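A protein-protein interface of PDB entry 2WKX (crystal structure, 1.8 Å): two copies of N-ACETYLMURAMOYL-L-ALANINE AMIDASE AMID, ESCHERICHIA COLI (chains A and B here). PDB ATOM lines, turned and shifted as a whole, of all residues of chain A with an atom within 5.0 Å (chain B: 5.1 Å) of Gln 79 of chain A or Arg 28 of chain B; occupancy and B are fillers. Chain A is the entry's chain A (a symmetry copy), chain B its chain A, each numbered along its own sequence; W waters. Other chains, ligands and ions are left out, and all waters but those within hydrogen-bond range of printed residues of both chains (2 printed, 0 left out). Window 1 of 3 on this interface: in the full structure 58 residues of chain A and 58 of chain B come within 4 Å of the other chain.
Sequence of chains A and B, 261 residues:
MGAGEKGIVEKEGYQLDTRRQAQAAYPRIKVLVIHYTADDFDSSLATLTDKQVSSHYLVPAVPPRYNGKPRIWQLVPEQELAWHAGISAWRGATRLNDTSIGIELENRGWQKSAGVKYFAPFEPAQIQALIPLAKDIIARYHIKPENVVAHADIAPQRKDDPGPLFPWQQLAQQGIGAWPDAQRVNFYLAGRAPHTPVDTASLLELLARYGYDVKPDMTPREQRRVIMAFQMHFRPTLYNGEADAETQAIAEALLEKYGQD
Arg 28 of chain B touches just these residues of chain A: Ile 29 (3.5 Å), His 56 (3.3 Å), Glu 78 (2.8 Å), Gln 79 (3.4 Å), Glu 80 (3.2 Å), Leu 81 (3.7 Å), Asn 97 (3.2 Å), Asp 98 (3.0 Å), Thr 99 (3.8 Å), Ser 100 (2.9 Å) and Ile 101 (3.96 Å). Printed residues of chain B within 4 Å of Ile 101 of chain A: Arg 28 (3.96 Å). Printed residues of chain B within 4 Å of Asn 97 of chain A: Arg 28 (3.2 Å). Printed residues of chain B within 4 Å of Thr 99 of chain A: Arg 28 (3.8 Å) and Asp 98 (3.5 Å). The nearest residue of chain B that does not touch Gln 79 of chain A is Tyr 26 of chain B (5.0 Å). The nearest residue of chain A that does not touch Arg 28 of chain B is Arg 28 of chain A (4.6 Å).
The backbone carbonyl oxygen (O) of Thr 99 of chain B is in hydrogen-bond range of the backbone NH (N) of Lys 30 of chain B, 2.8 Å away. The backbone carbonyl oxygen (O) of Glu 80 of chain A lies within hydrogen-bond range of a ring nitrogen (NE2) of His 56 of chain A, at 2.7 Å.
Arg 28 of chain A touches Ile 29 of chain B, and with the chains exchanged Ile 29 of chain A touches Arg 28 of chain B. Arg 28 of chain A touches Asp 98 of chain B, and with the chains exchanged Asp 98 of chain A touches Arg 28 of chain B. Arg 28 of chain A touches Thr 99 of chain B, and with the chains exchanged Thr 99 of chain A touches Arg 28 of chain B. Asp 98 of chain A touches Thr 99 of chain B, and with the chains exchanged Thr 99 of chain A touches Asp 98 of chain B. 4 positions are printed for both chains.
O of Tyr 26 of chain B lies within hydrogen-bond range of N of Leu 81 of chain A, 2.8 Å away. The guanidinium group (NH1) of Arg 28 of chain B lies within hydrogen-bond range of a ring nitrogen (NE2) of His 56 of chain A, 3.3 Å away. The guanidinium group (NH1) of Arg 28 of chain B sits at hydrogen-bond distance from the backbone carbonyl oxygen (O) of Glu 78 of chain A, at 2.8 Å. The backbone carbonyl oxygen (O) of Gln 79 of chain A sits at hydrogen-bond distance from the guanidinium group (NE) of Arg 28 of chain B (3.4 Å). The guanidinium group of Arg 28 of chain B lies within hydrogen-bond range of the backbone carbonyl oxygen of Glu 80 of chain A (3.2 Å). The backbone carbonyl oxygen (O) of Asn 97 of chain A sits at hydrogen-bond distance from the guanidinium group (NH2) of Arg 28 of chain B, at 3.2 Å. The backbone carbonyl oxygen (O) of Asp 98 of chain A lies within hydrogen-bond range of the guanidinium group (NH2) of Arg 28 of chain B (3.0 Å). O of Ser 100 of chain A sits at hydrogen-bond distance from NH2 of Arg 28 of chain B. The side-chain amino group (NZ) of Lys 30 of chain B lies within salt-bridge range of the side-chain carboxylate (OD1) of Asp 98 of chain A (2.8 Å). NH2 of Arg 28 of chain A is in hydrogen-bond range of O of Asp 98 of chain B.
Water W2 bridges the side-chain carboxylate (OD1) of Asp 98 of chain A and the side-chain amino group (NZ) of Lys 30 of chain B. Water W1 lies within hydrogen-bond range of the side-chain carboxylate (OD2) of Asp 98 of chain A (2.8 Å) and the side-chain amino group (NZ) of Lys 30 of chain B (3.0 Å).
Of the 7 printed residues of chain B, 7 touch a printed residue of chain A. Printed residues of chain B that touch a printed residue of chain A: Tyr 26, Pro 27, Arg 28, Ile 29, Lys 30, Asp 98 and Thr 99. Hydrophobic or aromatic side chains of chain B that line the printed part of chain A: Ile 29. Of the 13 printed residues of chain A, 12 touch a printed residue of chain B. Hydrophobic or aromatic side chains of chain A that line the printed part of chain B: Ile 29, His 56, Leu 81 and Ile 101. Among the printed residues, 21 pairs touch across the chains. Among the printed residues, Asp or Glu carboxylates within 4 Å of a Lys or Arg side-chain nitrogen of the other chain: Asp 98 of chain A with Lys 30 of chain B.
Ile 29 of chain B touches Arg 28 of chain A (CG1 to CZ, 3.5 Å). NH2 of Arg 28 of chain A touches N of Thr 99 of chain B (3.8 Å). Ile 29 of chain A touches Arg 28 of chain B (CG1 to CZ, 3.5 Å). O of Tyr 26 of chain B touches CB of Glu 80 of chain A, at 3.3 Å. CD2 of Leu 81 of chain A touches O of Pro 27 of chain B, at 3.5 Å. CG of Arg 28 of chain B touches N of Leu 81 of chain A (3.7 Å). Leu 81 of chain A touches Lys 30 of chain B. CG2 of Thr 99 of chain B touches OD2 of Asp 98 of chain A, 3.5 Å away. Thr 99 of chain A touches Asp 98 of chain B. Arg 28 of chain B touches Ile 101 of chain A (NH1 to CG1, 3.96 Å).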
ATOM      1  N   ARG A  28      31.270  -0.877  19.833  1.00  0.00           N
ATOM      2  CA  ARG A  28      29.946  -0.466  20.290  1.00  0.00           C
ATOM      3  C   ARG A  28      29.806  -0.708  21.808  1.00  0.00           C
ATOM      4  O   ARG A  28      28.951  -0.089  22.459  1.00  0.00           O
ATOM      5  CB  ARG A  28      28.873  -1.258  19.531  1.00  0.00           C
ATOM      6  CG  ARG A  28      28.858  -0.970  18.014  1.00  0.00           C
ATOM      7  CD  ARG A  28      27.785  -1.799  17.311  1.00  0.00           C
ATOM      8  NE  ARG A  28      27.848  -1.662  15.845  1.00  0.00           N
ATOM      9  CZ  ARG A  28      27.296  -0.678  15.119  1.00  0.00           C
ATOM     10  NH1 ARG A  28      27.457  -0.715  13.794  1.00  0.00           N
ATOM     11  NH2 ARG A  28      26.609   0.345  15.673  1.00  0.00           N
ATOM     12  N   ILE A  29      30.638  -1.614  22.338  1.00  0.00           N
ATOM     13  CA  ILE A  29      30.640  -1.959  23.787  1.00  0.00           C
ATOM     14  C   ILE A  29      31.597  -1.017  24.519  1.00  0.00           C
ATOM     15  O   ILE A  29      32.796  -0.993  24.223  1.00  0.00           O
ATOM     16  CB  ILE A  29      31.017  -3.441  24.009  1.00  0.00           C
ATOM     17  CG1 ILE A  29      29.922  -4.353  23.425  1.00  0.00           C
ATOM     18  CG2 ILE A  29      31.252  -3.750  25.500  1.00  0.00           C
ATOM     19  CD1 ILE A  29      30.415  -5.786  23.112  1.00  0.00           C
ATOM     20  N   HIS A  56      25.104 -11.256  30.138  1.00  0.00           N
ATOM     21  CA  HIS A  56      26.089 -12.000  29.345  1.00  0.00           C
ATOM     22  C   HIS A  56      26.760 -13.119  30.116  1.00  0.00           C
ATOM     23  O   HIS A  56      26.988 -14.211  29.568  1.00  0.00           O
ATOM     24  CB  HIS A  56      27.131 -11.060  28.758  1.00  0.00           C
ATOM     25  CG  HIS A  56      26.545 -10.061  27.801  1.00  0.00           C
ATOM     26  ND1 HIS A  56      26.101  -8.825  28.216  1.00  0.00           N
ATOM     27  CD2 HIS A  56      26.297 -10.133  26.468  1.00  0.00           C
ATOM     28  CE1 HIS A  56      25.623  -8.163  27.170  1.00  0.00           C
ATOM     29  NE2 HIS A  56      25.743  -8.932  26.095  1.00  0.00           N
ATOM     30  N   PRO A  77      25.883 -14.042  23.608  1.00  0.00           N
ATOM     31  CA  PRO A  77      27.105 -13.661  22.878  1.00  0.00           C
ATOM     32  C   PRO A  77      27.384 -12.181  23.111  1.00  0.00           C
ATOM     33  O   PRO A  77      26.442 -11.377  23.208  1.00  0.00           O
ATOM     34  CB  PRO A  77      26.760 -13.918  21.401  1.00  0.00           C
ATOM     35  CG  PRO A  77      25.561 -14.813  21.408  1.00  0.00           C
ATOM     36  CD  PRO A  77      24.831 -14.560  22.709  1.00  0.00           C
ATOM     37  N   GLU A  78      28.657 -11.805  23.214  1.00  0.00           N
ATOM     38  CA  GLU A  78      28.952 -10.400  23.555  1.00  0.00           C
ATOM     39  C   GLU A  78      28.472  -9.446  22.462  1.00  0.00           C
ATOM     40  O   GLU A  78      28.107  -8.302  22.766  1.00  0.00           O
ATOM     41  CB  GLU A  78      30.443 -10.194  23.816  1.00  0.00           C
ATOM     42  CG  GLU A  78      30.934 -10.892  25.103  1.00  0.00           C
ATOM     43  CD  GLU A  78      32.408 -10.650  25.383  1.00  0.00           C
ATOM     44  OE1 GLU A  78      33.146 -10.255  24.453  1.00  0.00           O
ATOM     45  OE2 GLU A  78      32.815 -10.867  26.546  1.00  0.00           O
ATOM     46  N   GLN A  79      28.429  -9.932  21.221  1.00  0.00           N
ATOM     47  CA  GLN A  79      27.993  -9.099  20.080  1.00  0.00           C
ATOM     48  C   GLN A  79      26.534  -8.648  20.228  1.00  0.00           C
ATOM     49  O   GLN A  79      26.159  -7.620  19.692  1.00  0.00           O
ATOM     50  CB  GLN A  79      28.191  -9.823  18.738  1.00  0.00           C
ATOM     51  CG  GLN A  79      27.095 -10.858  18.468  1.00  0.00           C
ATOM     52  CD  GLN A  79      27.527 -12.012  17.592  1.00  0.00           C
ATOM     53  OE1 GLN A  79      27.601 -13.164  18.048  1.00  0.00           O
ATOM     54  NE2 GLN A  79      27.811 -11.714  16.323  1.00  0.00           N
ATOM     55  N   GLU A  80      25.720  -9.426  20.945  1.00  0.00           N
ATOM     56  CA  GLU A  80      24.334  -9.074  21.217  1.00  0.00           C
ATOM     57  C   GLU A  80      24.147  -8.373  22.577  1.00  0.00           C
ATOM     58  O   GLU A  80      24.937  -8.579  23.500  1.00  0.00           O
ATOM     59  CB  GLU A  80      23.474 -10.337  21.177  1.00  0.00           C
ATOM     60  CG  GLU A  80      23.283 -10.922  19.769  1.00  0.00           C
ATOM     61  CD  GLU A  80      22.373 -12.139  19.802  1.00  0.00           C
ATOM     62  OE1 GLU A  80      21.279 -12.092  19.199  1.00  0.00           O
ATOM     63  OE2 GLU A  80      22.733 -13.131  20.456  1.00  0.00           O
ATOM     64  N   LEU A  81      23.103  -7.554  22.698  1.00  0.00           N
ATOM     65  CA  LEU A  81      22.732  -6.987  23.996  1.00  0.00           C
ATOM     66  C   LEU A  81      21.967  -8.038  24.820  1.00  0.00           C
ATOM     67  O   LEU A  81      21.239  -8.893  24.261  1.00  0.00           O
ATOM     68  CB  LEU A  81      21.938  -5.668  23.854  1.00  0.00           C
ATOM     69  CG  LEU A  81      20.549  -5.602  23.203  1.00  0.00           C
ATOM     70  CD1 LEU A  81      19.425  -5.962  24.212  1.00  0.00           C
ATOM     71  CD2 LEU A  81      20.278  -4.207  22.645  1.00  0.00           C
ATOM     72  N   ASN A  97      21.912  -1.101  28.180  1.00  0.00           N
ATOM     73  CA  ASN A  97      21.959  -2.418  27.502  1.00  0.00           C
ATOM     74  C   ASN A  97      22.663  -2.351  26.137  1.00  0.00           C
ATOM     75  O   ASN A  97      23.421  -3.261  25.776  1.00  0.00           O
ATOM     76  CB  ASN A  97      20.552  -2.983  27.268  1.00  0.00           C
ATOM     77  CG  ASN A  97      19.927  -3.533  28.536  1.00  0.00           C
ATOM     78  OD1 ASN A  97      20.624  -3.854  29.511  1.00  0.00           O
ATOM     79  ND2 ASN A  97      18.607  -3.670  28.509  1.00  0.00           N
ATOM     80  N   ASP A  98      22.425  -1.256  25.417  1.00  0.00           N
ATOM     81  CA  ASP A  98      22.865  -1.154  24.012  1.00  0.00           C
ATOM     82  C   ASP A  98      24.398  -1.212  23.906  1.00  0.00           C
ATOM     83  O   ASP A  98      24.926  -1.769  22.946  1.00  0.00           O
ATOM     84  CB  ASP A  98      22.381   0.165  23.394  1.00  0.00           C
ATOM     85  CG  ASP A  98      20.862   0.222  23.210  1.00  0.00           C
ATOM     86  OD1 ASP A  98      20.175  -0.804  23.443  1.00  0.00           O
ATOM     87  OD2 ASP A  98      20.376   1.298  22.812  1.00  0.00           O
ATOM     88  N   THR A  99      25.082  -0.609  24.877  1.00  0.00           N
ATOM     89  CA  THR A  99      26.539  -0.378  24.829  1.00  0.00           C
ATOM     90  C   THR A  99      27.274  -1.039  26.005  1.00  0.00           C
ATOM     91  O   THR A  99      28.425  -0.694  26.296  1.00  0.00           O
ATOM     92  CB  THR A  99      26.880   1.140  24.815  1.00  0.00           C
ATOM     93  OG1 THR A  99      26.262   1.785  25.946  1.00  0.00           O
ATOM     94  CG2 THR A  99      26.388   1.780  23.496  1.00  0.00           C
ATOM     95  N   SER A 100      26.625  -1.989  26.669  1.00  0.00           N
ATOM     96  CA  SER A 100      27.304  -2.667  27.795  1.00  0.00           C
ATOM     97  C   SER A 100      27.350  -4.183  27.707  1.00  0.00           C
ATOM     98  O   SER A 100      26.582  -4.810  26.959  1.00  0.00           O
ATOM     99  CB  SER A 100      26.686  -2.288  29.149  1.00  0.00           C
ATOM    100  OG  SER A 100      25.355  -2.809  29.256  1.00  0.00           O
ATOM    101  N   ILE A 101      28.256  -4.738  28.508  1.00  0.00           N
ATOM    102  CA  ILE A 101      28.247  -6.156  28.880  1.00  0.00           C
ATOM    103  C   ILE A 101      27.813  -6.232  30.356  1.00  0.00           C
ATOM    104  O   ILE A 101      28.241  -5.417  31.195  1.00  0.00           O
ATOM    105  CB  ILE A 101      29.635  -6.813  28.638  1.00  0.00           C
ATOM    106  CG1 ILE A 101      29.870  -6.989  27.115  1.00  0.00           C
ATOM    107  CG2 ILE A 101      29.749  -8.160  29.386  1.00  0.00           C
ATOM    108  CD1 ILE A 101      31.261  -7.472  26.771  1.00  0.00           C
ATOM    109  N   TYR B  26      19.502  -9.806  21.768  1.00  0.00           N
ATOM    110  CA  TYR B  26      19.096  -9.021  20.598  1.00  0.00           C
ATOM    111  C   TYR B  26      20.272  -8.261  19.991  1.00  0.00           C
ATOM    112  O   TYR B  26      21.252  -7.986  20.710  1.00  0.00           O
ATOM    113  CB  TYR B  26      17.988  -8.029  20.986  1.00  0.00           C
ATOM    114  CG  TYR B  26      16.772  -8.726  21.560  1.00  0.00           C
ATOM    115  CD1 TYR B  26      16.594  -8.833  22.943  1.00  0.00           C
ATOM    116  CD2 TYR B  26      15.814  -9.311  20.716  1.00  0.00           C
ATOM    117  CE1 TYR B  26      15.474  -9.512  23.479  1.00  0.00           C
ATOM    118  CE2 TYR B  26      14.699  -9.984  21.239  1.00  0.00           C
ATOM    119  CZ  TYR B  26      14.545 -10.073  22.621  1.00  0.00           C
ATOM    120  OH  TYR B  26      13.453 -10.718  23.144  1.00  0.00           O
ATOM    121  N   PRO B  27      20.178  -7.896  18.690  1.00  0.00           N
ATOM    122  CA  PRO B  27      21.240  -7.093  18.077  1.00  0.00           C
ATOM    123  C   PRO B  27      21.428  -5.763  18.801  1.00  0.00           C
ATOM    124  O   PRO B  27      20.452  -5.178  19.299  1.00  0.00           O
ATOM    125  CB  PRO B  27      20.743  -6.861  16.635  1.00  0.00           C
ATOM    126  CG  PRO B  27      19.767  -8.000  16.374  1.00  0.00           C
ATOM    127  CD  PRO B  27      19.109  -8.232  17.724  1.00  0.00           C
ATOM    128  N   ARG B  28      22.675  -5.310  18.869  1.00  0.00           N
ATOM    129  CA  ARG B  28      22.986  -3.951  19.303  1.00  0.00           C
ATOM    130  C   ARG B  28      22.690  -2.946  18.169  1.00  0.00           C
ATOM    131  O   ARG B  28      22.506  -1.749  18.433  1.00  0.00           O
ATOM    132  CB  ARG B  28      24.465  -3.869  19.705  1.00  0.00           C
ATOM    133  CG  ARG B  28      24.818  -4.747  20.924  1.00  0.00           C
ATOM    134  CD  ARG B  28      26.303  -4.638  21.264  1.00  0.00           C
ATOM    135  NE  ARG B  28      26.702  -5.582  22.324  1.00  0.00           N
ATOM    136  CZ  ARG B  28      26.578  -5.385  23.645  1.00  0.00           C
ATOM    137  NH1 ARG B  28      26.994  -6.356  24.463  1.00  0.00           N
ATOM    138  NH2 ARG B  28      26.038  -4.264  24.170  1.00  0.00           N
ATOM    139  N   ILE B  29      22.664  -3.451  16.928  1.00  0.00           N
ATOM    140  CA  ILE B  29      22.385  -2.621  15.725  1.00  0.00           C
ATOM    141  C   ILE B  29      20.875  -2.596  15.479  1.00  0.00           C
ATOM    142  O   ILE B  29      20.263  -3.646  15.258  1.00  0.00           O
ATOM    143  CB  ILE B  29      23.155  -3.144  14.492  1.00  0.00           C
ATOM    144  CG1 ILE B  29      24.670  -2.965  14.707  1.00  0.00           C
ATOM    145  CG2 ILE B  29      22.697  -2.445  13.197  1.00  0.00           C
ATOM    146  CD1 ILE B  29      25.533  -3.901  13.825  1.00  0.00           C
ATOM    147  N   LYS B  30      20.288  -1.401  15.547  1.00  0.00           N
ATOM    148  CA  LYS B  30      18.829  -1.235  15.420  1.00  0.00           C
ATOM    149  C   LYS B  30      18.362  -0.268  14.317  1.00  0.00           C
ATOM    150  O   LYS B  30      17.162  -0.215  14.007  1.00  0.00           O
ATOM    151  CB  LYS B  30      18.276  -0.699  16.733  1.00  0.00           C
ATOM    152  CG  LYS B  30      18.632  -1.564  17.943  1.00  0.00           C
ATOM    153  CD  LYS B  30      18.155  -0.896  19.197  1.00  0.00           C
ATOM    154  CE  LYS B  30      18.708  -1.664  20.388  1.00  0.00           C
ATOM    155  NZ  LYS B  30      18.108  -1.141  21.636  1.00  0.00           N
ATOM    156  N   ASP B  98      26.094   4.550  18.061  1.00  0.00           N
ATOM    157  CA  ASP B  98      26.275   3.364  18.919  1.00  0.00           C
ATOM    158  C   ASP B  98      25.458   2.171  18.396  1.00  0.00           C
ATOM    159  O   ASP B  98      25.902   1.029  18.500  1.00  0.00           O
ATOM    160  CB  ASP B  98      25.831   3.669  20.357  1.00  0.00           C
ATOM    161  CG  ASP B  98      26.746   4.666  21.071  1.00  0.00           C
ATOM    162  OD1 ASP B  98      27.806   5.041  20.510  1.00  0.00           O
ATOM    163  OD2 ASP B  98      26.397   5.048  22.204  1.00  0.00           O
ATOM    164  N   THR B  99      24.267   2.454  17.872  1.00  0.00           N
ATOM    165  CA  THR B  99      23.263   1.431  17.519  1.00  0.00           C
ATOM    166  C   THR B  99      22.882   1.473  16.032  1.00  0.00           C
ATOM    167  O   THR B  99      21.853   0.916  15.635  1.00  0.00           O
ATOM    168  CB  THR B  99      21.971   1.576  18.373  1.00  0.00           C
ATOM    169  OG1 THR B  99      21.453   2.915  18.241  1.00  0.00           O
ATOM    170  CG2 THR B  99      22.276   1.262  19.855  1.00  0.00           C
HETATM  171  O   HOH W   1      18.096   1.891  21.315  1.00  0.00           O
HETATM  172  O   HOH W   2      17.909  -0.883  24.972  1.00  0.00           O
